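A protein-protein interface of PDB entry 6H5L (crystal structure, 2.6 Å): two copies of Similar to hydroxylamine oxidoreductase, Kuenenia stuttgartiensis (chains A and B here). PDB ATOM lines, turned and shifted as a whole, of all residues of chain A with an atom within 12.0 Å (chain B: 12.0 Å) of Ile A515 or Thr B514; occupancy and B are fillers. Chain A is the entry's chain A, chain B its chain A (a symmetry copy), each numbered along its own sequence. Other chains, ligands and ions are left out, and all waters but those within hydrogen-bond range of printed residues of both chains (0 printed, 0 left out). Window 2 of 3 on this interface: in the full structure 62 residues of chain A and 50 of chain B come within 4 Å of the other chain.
The side-chain carboxylate (OE2) of Glu A512 lies within salt-bridge range of the guanidinium group (NE) of Arg B507.
The backbone carbonyl oxygen (O) of Gly B510 lies within hydrogen-bond range of the side-chain hydroxyl (OG1) of Thr B514 (3.1 Å).
OG1 of Thr B514 sits at hydrogen-bond distance from O of Ile B511.
Tyr A394 touches Arg B507 (CB to NH1, 3.4 Å).
Arg B507 touches Leu A508 (CD to CD2, 3.7 Å).
Leu A508 touches Leu B508 (CD2 to CD1, 3.95 Å).
Glu A512 touches Ile B511.
OG1 of Thr B514 touches CD1 of Ile A515 (3.5 Å).
Printed residues of chain B within 4 Å of Tyr A394: Arg B507.
Of chain B, only Arg B507 and Ile B511 come within 4 Å of Glu A512.
No residue of chain B comes within 4 Å of Thr A514.
Of chain B, only Thr B514 comes within 4 Å of Ile A515.
Of the printed residues of chain A, Arg B507 touches Tyr A394 (3.4 Å), Leu A508 (3.7 Å) and Glu A512 (2.6 Å).
Printed residues of chain A within 4 Å of Leu B508: Leu A508 (3.95 Å).
No residue of chain A comes within 4 Å of Gly B510.
Printed residues of chain A within 4 Å of Ile B511: Glu A512 (3.7 Å).
No residue of chain A comes within 4 Å of Lys B513.
Thr B514 touches just one residue of chain A: Ile A515 (3.5 Å).
No residue of chain A comes within 4 Å of Ile B515.
No residue of chain A comes within 4 Å of Ser B516.
The nearest residue of chain A that does not touch Thr B514 is Ser A516 (7.5 Å).
The nearest printed residue of chain B that does not touch Tyr A394 is Arg B506 (5.3 Å).
Of the 13 printed residues of chain B, 4 touch a printed residue of chain A.
Of the 12 printed residues of chain A, 4 touch a printed residue of chain B.
Printed residues of chain A that touch a printed residue of chain B: Tyr A394, Leu A508, Glu A512 and Ile A515.
Hydrophobic or aromatic side chains of chain A that line the printed part of chain B: Tyr A394, Leu A508 and Ile A515.
Among the printed residues, 6 pairs touch across the chains.
Among the printed residues, Asp or Glu carboxylates within 4 Å of a Lys or Arg side-chain nitrogen of the other chain: Glu A512 with Arg B507.
Leu A508 touches Arg B507, but with the chains exchanged Arg A507 does not touch Leu B508 (8.5 Å).
Leu A508 touches its own counterpart, Leu B508.
Glu A512 touches Arg B507, but with the chains exchanged Arg A507 does not touch Glu B512 (12.2 Å).
Ile A515 touches Thr B514, but with the chains exchanged Thr A514 does not touch Ile B515 (8.0 Å).
Of the 6 pairs that touch across the chains among the printed residues, 1 has its exchanged pair printed and touching as well.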
ATOM      1  N   TYR A 394       9.276  25.679 -21.794  1.00  0.00           N
ATOM      2  CA  TYR A 394       8.640  24.790 -20.826  1.00  0.00           C
ATOM      3  C   TYR A 394       7.824  25.614 -19.839  1.00  0.00           C
ATOM      4  O   TYR A 394       8.389  26.485 -19.147  1.00  0.00           O
ATOM      5  CB  TYR A 394       9.679  23.938 -20.095  1.00  0.00           C
ATOM      6  CG  TYR A 394       9.077  22.960 -19.111  1.00  0.00           C
ATOM      7  CD1 TYR A 394       8.556  21.744 -19.538  1.00  0.00           C
ATOM      8  CD2 TYR A 394       9.029  23.252 -17.755  1.00  0.00           C
ATOM      9  CE1 TYR A 394       8.003  20.847 -18.640  1.00  0.00           C
ATOM     10  CE2 TYR A 394       8.479  22.362 -16.850  1.00  0.00           C
ATOM     11  CZ  TYR A 394       7.968  21.162 -17.298  1.00  0.00           C
ATOM     12  OH  TYR A 394       7.421  20.277 -16.398  1.00  0.00           O
ATOM     13  N   ARG A 506      18.388  24.427 -22.446  1.00  0.00           N
ATOM     14  CA  ARG A 506      19.068  23.473 -23.315  1.00  0.00           C
ATOM     15  C   ARG A 506      19.782  22.403 -22.498  1.00  0.00           C
ATOM     16  O   ARG A 506      19.861  21.242 -22.916  1.00  0.00           O
ATOM     17  CB  ARG A 506      20.052  24.201 -24.231  1.00  0.00           C
ATOM     18  CG  ARG A 506      19.399  25.247 -25.111  1.00  0.00           C
ATOM     19  CD  ARG A 506      20.387  25.898 -26.062  1.00  0.00           C
ATOM     20  NE  ARG A 506      19.732  26.903 -26.895  1.00  0.00           N
ATOM     21  CZ  ARG A 506      19.062  26.629 -28.010  1.00  0.00           C
ATOM     22  NH1 ARG A 506      18.960  25.376 -28.432  1.00  0.00           N
ATOM     23  NH2 ARG A 506      18.492  27.605 -28.702  1.00  0.00           N
ATOM     24  N   ARG A 507      20.308  22.779 -21.329  1.00  0.00           N
ATOM     25  CA  ARG A 507      20.970  21.813 -20.459  1.00  0.00           C
ATOM     26  C   ARG A 507      19.980  20.787 -19.922  1.00  0.00           C
ATOM     27  O   ARG A 507      20.271  19.585 -19.898  1.00  0.00           O
ATOM     28  CB  ARG A 507      21.665  22.544 -19.311  1.00  0.00           C
ATOM     29  CG  ARG A 507      22.485  21.653 -18.399  1.00  0.00           C
ATOM     30  CD  ARG A 507      23.110  22.469 -17.281  1.00  0.00           C
ATOM     31  NE  ARG A 507      24.069  21.702 -16.491  1.00  0.00           N
ATOM     32  CZ  ARG A 507      24.741  22.196 -15.457  1.00  0.00           C
ATOM     33  NH1 ARG A 507      24.559  23.457 -15.087  1.00  0.00           N
ATOM     34  NH2 ARG A 507      25.596  21.432 -14.793  1.00  0.00           N
ATOM     35  N   LEU A 508      18.805  21.245 -19.485  1.00  0.00           N
ATOM     36  CA  LEU A 508      17.787  20.325 -18.989  1.00  0.00           C
ATOM     37  C   LEU A 508      17.308  19.385 -20.086  1.00  0.00           C
ATOM     38  O   LEU A 508      17.099  18.190 -19.842  1.00  0.00           O
ATOM     39  CB  LEU A 508      16.610  21.108 -18.405  1.00  0.00           C
ATOM     40  CG  LEU A 508      16.475  21.118 -16.881  1.00  0.00           C
ATOM     41  CD1 LEU A 508      17.751  21.614 -16.214  1.00  0.00           C
ATOM     42  CD2 LEU A 508      15.286  21.964 -16.455  1.00  0.00           C
ATOM     43  N   ALA A 509      17.123  19.905 -21.301  1.00  0.00           N
ATOM     44  CA  ALA A 509      16.675  19.060 -22.402  1.00  0.00           C
ATOM     45  C   ALA A 509      17.744  18.049 -22.798  1.00  0.00           C
ATOM     46  O   ALA A 509      17.427  16.904 -23.135  1.00  0.00           O
ATOM     47  CB  ALA A 509      16.283  19.922 -23.601  1.00  0.00           C
ATOM     48  N   GLY A 510      19.017  18.452 -22.757  1.00  0.00           N
ATOM     49  CA  GLY A 510      20.104  17.524 -23.022  1.00  0.00           C
ATOM     50  C   GLY A 510      20.198  16.388 -22.027  1.00  0.00           C
ATOM     51  O   GLY A 510      20.864  15.385 -22.305  1.00  0.00           O
ATOM     52  N   ILE A 511      19.548  16.524 -20.874  1.00  0.00           N
ATOM     53  CA  ILE A 511      19.459  15.447 -19.894  1.00  0.00           C
ATOM     54  C   ILE A 511      18.201  14.615 -20.102  1.00  0.00           C
ATOM     55  O   ILE A 511      18.234  13.388 -19.978  1.00  0.00           O
ATOM     56  CB  ILE A 511      19.522  16.035 -18.469  1.00  0.00           C
ATOM     57  CG1 ILE A 511      20.944  16.521 -18.160  1.00  0.00           C
ATOM     58  CG2 ILE A 511      19.029  15.025 -17.432  1.00  0.00           C
ATOM     59  CD1 ILE A 511      21.079  17.228 -16.828  1.00  0.00           C
ATOM     60  N   GLU A 512      17.082  15.265 -20.435  1.00  0.00           N
ATOM     61  CA  GLU A 512      15.844  14.538 -20.697  1.00  0.00           C
ATOM     62  C   GLU A 512      15.941  13.652 -21.931  1.00  0.00           C
ATOM     63  O   GLU A 512      15.089  12.777 -22.117  1.00  0.00           O
ATOM     64  CB  GLU A 512      14.675  15.515 -20.858  1.00  0.00           C
ATOM     65  CG  GLU A 512      14.369  16.332 -19.616  1.00  0.00           C
ATOM     66  CD  GLU A 512      13.252  17.334 -19.832  1.00  0.00           C
ATOM     67  OE1 GLU A 512      12.767  17.453 -20.976  1.00  0.00           O
ATOM     68  OE2 GLU A 512      12.860  18.004 -18.854  1.00  0.00           O
ATOM     69  N   LYS A 513      16.951  13.858 -22.776  1.00  0.00           N
ATOM     70  CA  LYS A 513      17.148  13.000 -23.934  1.00  0.00           C
ATOM     71  C   LYS A 513      18.022  11.796 -23.611  1.00  0.00           C
ATOM     72  O   LYS A 513      17.706  10.675 -24.028  1.00  0.00           O
ATOM     73  CB  LYS A 513      17.760  13.796 -25.091  1.00  0.00           C
ATOM     74  CG  LYS A 513      17.956  12.970 -26.350  1.00  0.00           C
ATOM     75  CD  LYS A 513      18.301  13.844 -27.540  1.00  0.00           C
ATOM     76  CE  LYS A 513      18.364  13.028 -28.822  1.00  0.00           C
ATOM     77  NZ  LYS A 513      18.585  13.876 -30.028  1.00  0.00           N
ATOM     78  N   THR A 514      19.111  11.998 -22.859  1.00  0.00           N
ATOM     79  CA  THR A 514      19.982  10.903 -22.447  1.00  0.00           C
ATOM     80  C   THR A 514      19.444  10.150 -21.236  1.00  0.00           C
ATOM     81  O   THR A 514      20.199   9.416 -20.583  1.00  0.00           O
ATOM     82  CB  THR A 514      21.396  11.417 -22.151  1.00  0.00           C
ATOM     83  OG1 THR A 514      21.332  12.482 -21.193  1.00  0.00           O
ATOM     84  CG2 THR A 514      22.068  11.925 -23.426  1.00  0.00           C
ATOM     85  N   ILE A 515      18.161  10.328 -20.925  1.00  0.00           N
ATOM     86  CA  ILE A 515      17.452   9.533 -19.930  1.00  0.00           C
ATOM     87  C   ILE A 515      16.444   8.598 -20.572  1.00  0.00           C
ATOM     88  O   ILE A 515      15.746   7.861 -19.856  1.00  0.00           O
ATOM     89  CB  ILE A 515      16.761  10.434 -18.890  1.00  0.00           C
ATOM     90  CG1 ILE A 515      16.531   9.661 -17.587  1.00  0.00           C
ATOM     91  CG2 ILE A 515      15.457  10.997 -19.468  1.00  0.00           C
ATOM     92  CD1 ILE A 515      15.912  10.472 -16.465  1.00  0.00           C
ATOM     93  N   SER A 516      16.332   8.619 -21.899  1.00  0.00           N
ATOM     94  CA  SER A 516      15.434   7.739 -22.637  1.00  0.00           C
ATOM     95  C   SER A 516      16.127   6.408 -22.923  1.00  0.00           C
ATOM     96  O   SER A 516      15.458   5.378 -22.959  1.00  0.00           O
ATOM     97  CB  SER A 516      14.954   8.416 -23.940  1.00  0.00           C
ATOM     98  OG  SER A 516      14.381   9.700 -23.680  1.00  0.00           O
ATOM     99  N   LEU B 392       8.747  19.441  -2.479  1.00  0.00           N
ATOM    100  CA  LEU B 392       9.580  19.857  -3.593  1.00  0.00           C
ATOM    101  C   LEU B 392      10.476  21.040  -3.253  1.00  0.00           C
ATOM    102  O   LEU B 392      11.301  21.434  -4.082  1.00  0.00           O
ATOM    103  CB  LEU B 392       8.704  20.186  -4.804  1.00  0.00           C
ATOM    104  CG  LEU B 392       7.795  19.031  -5.236  1.00  0.00           C
ATOM    105  CD1 LEU B 392       6.919  19.449  -6.397  1.00  0.00           C
ATOM    106  CD2 LEU B 392       8.606  17.794  -5.597  1.00  0.00           C
ATOM    107  N   LEU B 505      10.852  23.240 -10.262  1.00  0.00           N
ATOM    108  CA  LEU B 505      11.079  22.287  -9.181  1.00  0.00           C
ATOM    109  C   LEU B 505      10.334  20.980  -9.413  1.00  0.00           C
ATOM    110  O   LEU B 505      10.821  19.914  -9.019  1.00  0.00           O
ATOM    111  CB  LEU B 505      10.670  22.904  -7.845  1.00  0.00           C
ATOM    112  CG  LEU B 505      11.564  24.038  -7.341  1.00  0.00           C
ATOM    113  CD1 LEU B 505      10.929  24.737  -6.151  1.00  0.00           C
ATOM    114  CD2 LEU B 505      12.943  23.507  -6.978  1.00  0.00           C
ATOM    115  N   ARG B 506       9.157  21.035 -10.043  1.00  0.00           N
ATOM    116  CA  ARG B 506       8.450  19.804 -10.378  1.00  0.00           C
ATOM    117  C   ARG B 506       9.135  19.077 -11.529  1.00  0.00           C
ATOM    118  O   ARG B 506       9.148  17.841 -11.570  1.00  0.00           O
ATOM    119  CB  ARG B 506       6.993  20.111 -10.723  1.00  0.00           C
ATOM    120  CG  ARG B 506       6.235  20.791  -9.601  1.00  0.00           C
ATOM    121  CD  ARG B 506       4.773  21.014  -9.945  1.00  0.00           C
ATOM    122  NE  ARG B 506       4.069  21.674  -8.848  1.00  0.00           N
ATOM    123  CZ  ARG B 506       3.573  21.041  -7.790  1.00  0.00           C
ATOM    124  NH1 ARG B 506       3.701  19.725  -7.683  1.00  0.00           N
ATOM    125  NH2 ARG B 506       2.953  21.721  -6.836  1.00  0.00           N
ATOM    126  N   ARG B 507       9.709  19.829 -12.471  1.00  0.00           N
ATOM    127  CA  ARG B 507      10.425  19.219 -13.585  1.00  0.00           C
ATOM    128  C   ARG B 507      11.679  18.498 -13.103  1.00  0.00           C
ATOM    129  O   ARG B 507      11.964  17.376 -13.538  1.00  0.00           O
ATOM    130  CB  ARG B 507      10.782  20.289 -14.615  1.00  0.00           C
ATOM    131  CG  ARG B 507      11.434  19.758 -15.877  1.00  0.00           C
ATOM    132  CD  ARG B 507      11.771  20.899 -16.822  1.00  0.00           C
ATOM    133  NE  ARG B 507      12.216  20.433 -18.132  1.00  0.00           N
ATOM    134  CZ  ARG B 507      12.570  21.242 -19.125  1.00  0.00           C
ATOM    135  NH1 ARG B 507      12.534  22.557 -18.956  1.00  0.00           N
ATOM    136  NH2 ARG B 507      12.961  20.738 -20.286  1.00  0.00           N
ATOM    137  N   LEU B 508      12.438  19.129 -12.204  1.00  0.00           N
ATOM    138  CA  LEU B 508      13.635  18.492 -11.666  1.00  0.00           C
ATOM    139  C   LEU B 508      13.288  17.238 -10.876  1.00  0.00           C
ATOM    140  O   LEU B 508      13.986  16.222 -10.971  1.00  0.00           O
ATOM    141  CB  LEU B 508      14.406  19.480 -10.787  1.00  0.00           C
ATOM    142  CG  LEU B 508      15.705  20.047 -11.362  1.00  0.00           C
ATOM    143  CD1 LEU B 508      15.473  20.700 -12.717  1.00  0.00           C
ATOM    144  CD2 LEU B 508      16.331  21.036 -10.392  1.00  0.00           C
ATOM    145  N   ALA B 509      12.212  17.289 -10.086  1.00  0.00           N
ATOM    146  CA  ALA B 509      11.814  16.121  -9.310  1.00  0.00           C
ATOM    147  C   ALA B 509      11.325  14.994 -10.212  1.00  0.00           C
ATOM    148  O   ALA B 509      11.587  13.817  -9.939  1.00  0.00           O
ATOM    149  CB  ALA B 509      10.736  16.504  -8.297  1.00  0.00           C
ATOM    150  N   GLY B 510      10.618  15.333 -11.292  1.00  0.00           N
ATOM    151  CA  GLY B 510      10.198  14.331 -12.256  1.00  0.00           C
ATOM    152  C   GLY B 510      11.345  13.630 -12.953  1.00  0.00           C
ATOM    153  O   GLY B 510      11.140  12.569 -13.552  1.00  0.00           O
ATOM    154  N   ILE B 511      12.545  14.200 -12.888  1.00  0.00           N
ATOM    155  CA  ILE B 511      13.747  13.557 -13.407  1.00  0.00           C
ATOM    156  C   ILE B 511      14.456  12.756 -12.323  1.00  0.00           C
ATOM    157  O   ILE B 511      14.954  11.657 -12.581  1.00  0.00           O
ATOM    158  CB  ILE B 511      14.677  14.619 -14.030  1.00  0.00           C
ATOM    159  CG1 ILE B 511      14.089  15.127 -15.352  1.00  0.00           C
ATOM    160  CG2 ILE B 511      16.095  14.073 -14.211  1.00  0.00           C
ATOM    161  CD1 ILE B 511      14.870  16.263 -15.978  1.00  0.00           C
ATOM    162  N   GLU B 512      14.498  13.284 -11.097  1.00  0.00           N
ATOM    163  CA  GLU B 512      15.118  12.561  -9.991  1.00  0.00           C
ATOM    164  C   GLU B 512      14.367  11.286  -9.638  1.00  0.00           C
ATOM    165  O   GLU B 512      14.916  10.436  -8.927  1.00  0.00           O
ATOM    166  CB  GLU B 512      15.215  13.459  -8.753  1.00  0.00           C
ATOM    167  CG  GLU B 512      16.094  14.682  -8.935  1.00  0.00           C
ATOM    168  CD  GLU B 512      16.112  15.580  -7.715  1.00  0.00           C
ATOM    169  OE1 GLU B 512      15.372  15.295  -6.750  1.00  0.00           O
ATOM    170  OE2 GLU B 512      16.868  16.575  -7.722  1.00  0.00           O
ATOM    171  N   LYS B 513      13.132  11.131 -10.111  1.00  0.00           N
ATOM    172  CA  LYS B 513      12.384   9.904  -9.878  1.00  0.00           C
ATOM    173  C   LYS B 513      12.638   8.866 -10.962  1.00  0.00           C
ATOM    174  O   LYS B 513      12.826   7.683 -10.652  1.00  0.00           O
ATOM    175  CB  LYS B 513      10.886  10.201  -9.777  1.00  0.00           C
ATOM    176  CG  LYS B 513      10.048   8.968  -9.491  1.00  0.00           C
ATOM    177  CD  LYS B 513       8.622   9.336  -9.128  1.00  0.00           C
ATOM    178  CE  LYS B 513       7.825   8.110  -8.715  1.00  0.00           C
ATOM    179  NZ  LYS B 513       6.454   8.453  -8.240  1.00  0.00           N
ATOM    180  N   THR B 514      12.663   9.284 -12.233  1.00  0.00           N
ATOM    181  CA  THR B 514      12.953   8.379 -13.340  1.00  0.00           C
ATOM    182  C   THR B 514      14.447   8.138 -13.526  1.00  0.00           C
ATOM    183  O   THR B 514      14.866   7.662 -14.589  1.00  0.00           O
ATOM    184  CB  THR B 514      12.349   8.909 -14.646  1.00  0.00           C
ATOM    185  OG1 THR B 514      12.799  10.251 -14.877  1.00  0.00           O
ATOM    186  CG2 THR B 514      10.821   8.893 -14.585  1.00  0.00           C
ATOM    187  N   ILE B 515      15.250   8.467 -12.515  1.00  0.00           N
ATOM    188  CA  ILE B 515      16.662   8.116 -12.456  1.00  0.00           C
ATOM    189  C   ILE B 515      16.935   7.053 -11.409  1.00  0.00           C
ATOM    190  O   ILE B 515      18.096   6.653 -11.225  1.00  0.00           O
ATOM    191  CB  ILE B 515      17.533   9.359 -12.196  1.00  0.00           C
ATOM    192  CG1 ILE B 515      18.962   9.121 -12.697  1.00  0.00           C
ATOM    193  CG2 ILE B 515      17.494   9.725 -10.708  1.00  0.00           C
ATOM    194  CD1 ILE B 515      19.895  10.307 -12.551  1.00  0.00           C
ATOM    195  N   SER B 516      15.902   6.595 -10.703  1.00  0.00           N
ATOM    196  CA  SER B 516      16.025   5.544  -9.701  1.00  0.00           C
ATOM    197  C   SER B 516      15.912   4.174 -10.366  1.00  0.00           C
ATOM    198  O   SER B 516      16.548   3.227  -9.906  1.00  0.00           O
ATOM    199  CB  SER B 516      14.967   5.720  -8.589  1.00  0.00           C
ATOM    200  OG  SER B 516      15.018   7.032  -8.024  1.00  0.00           O
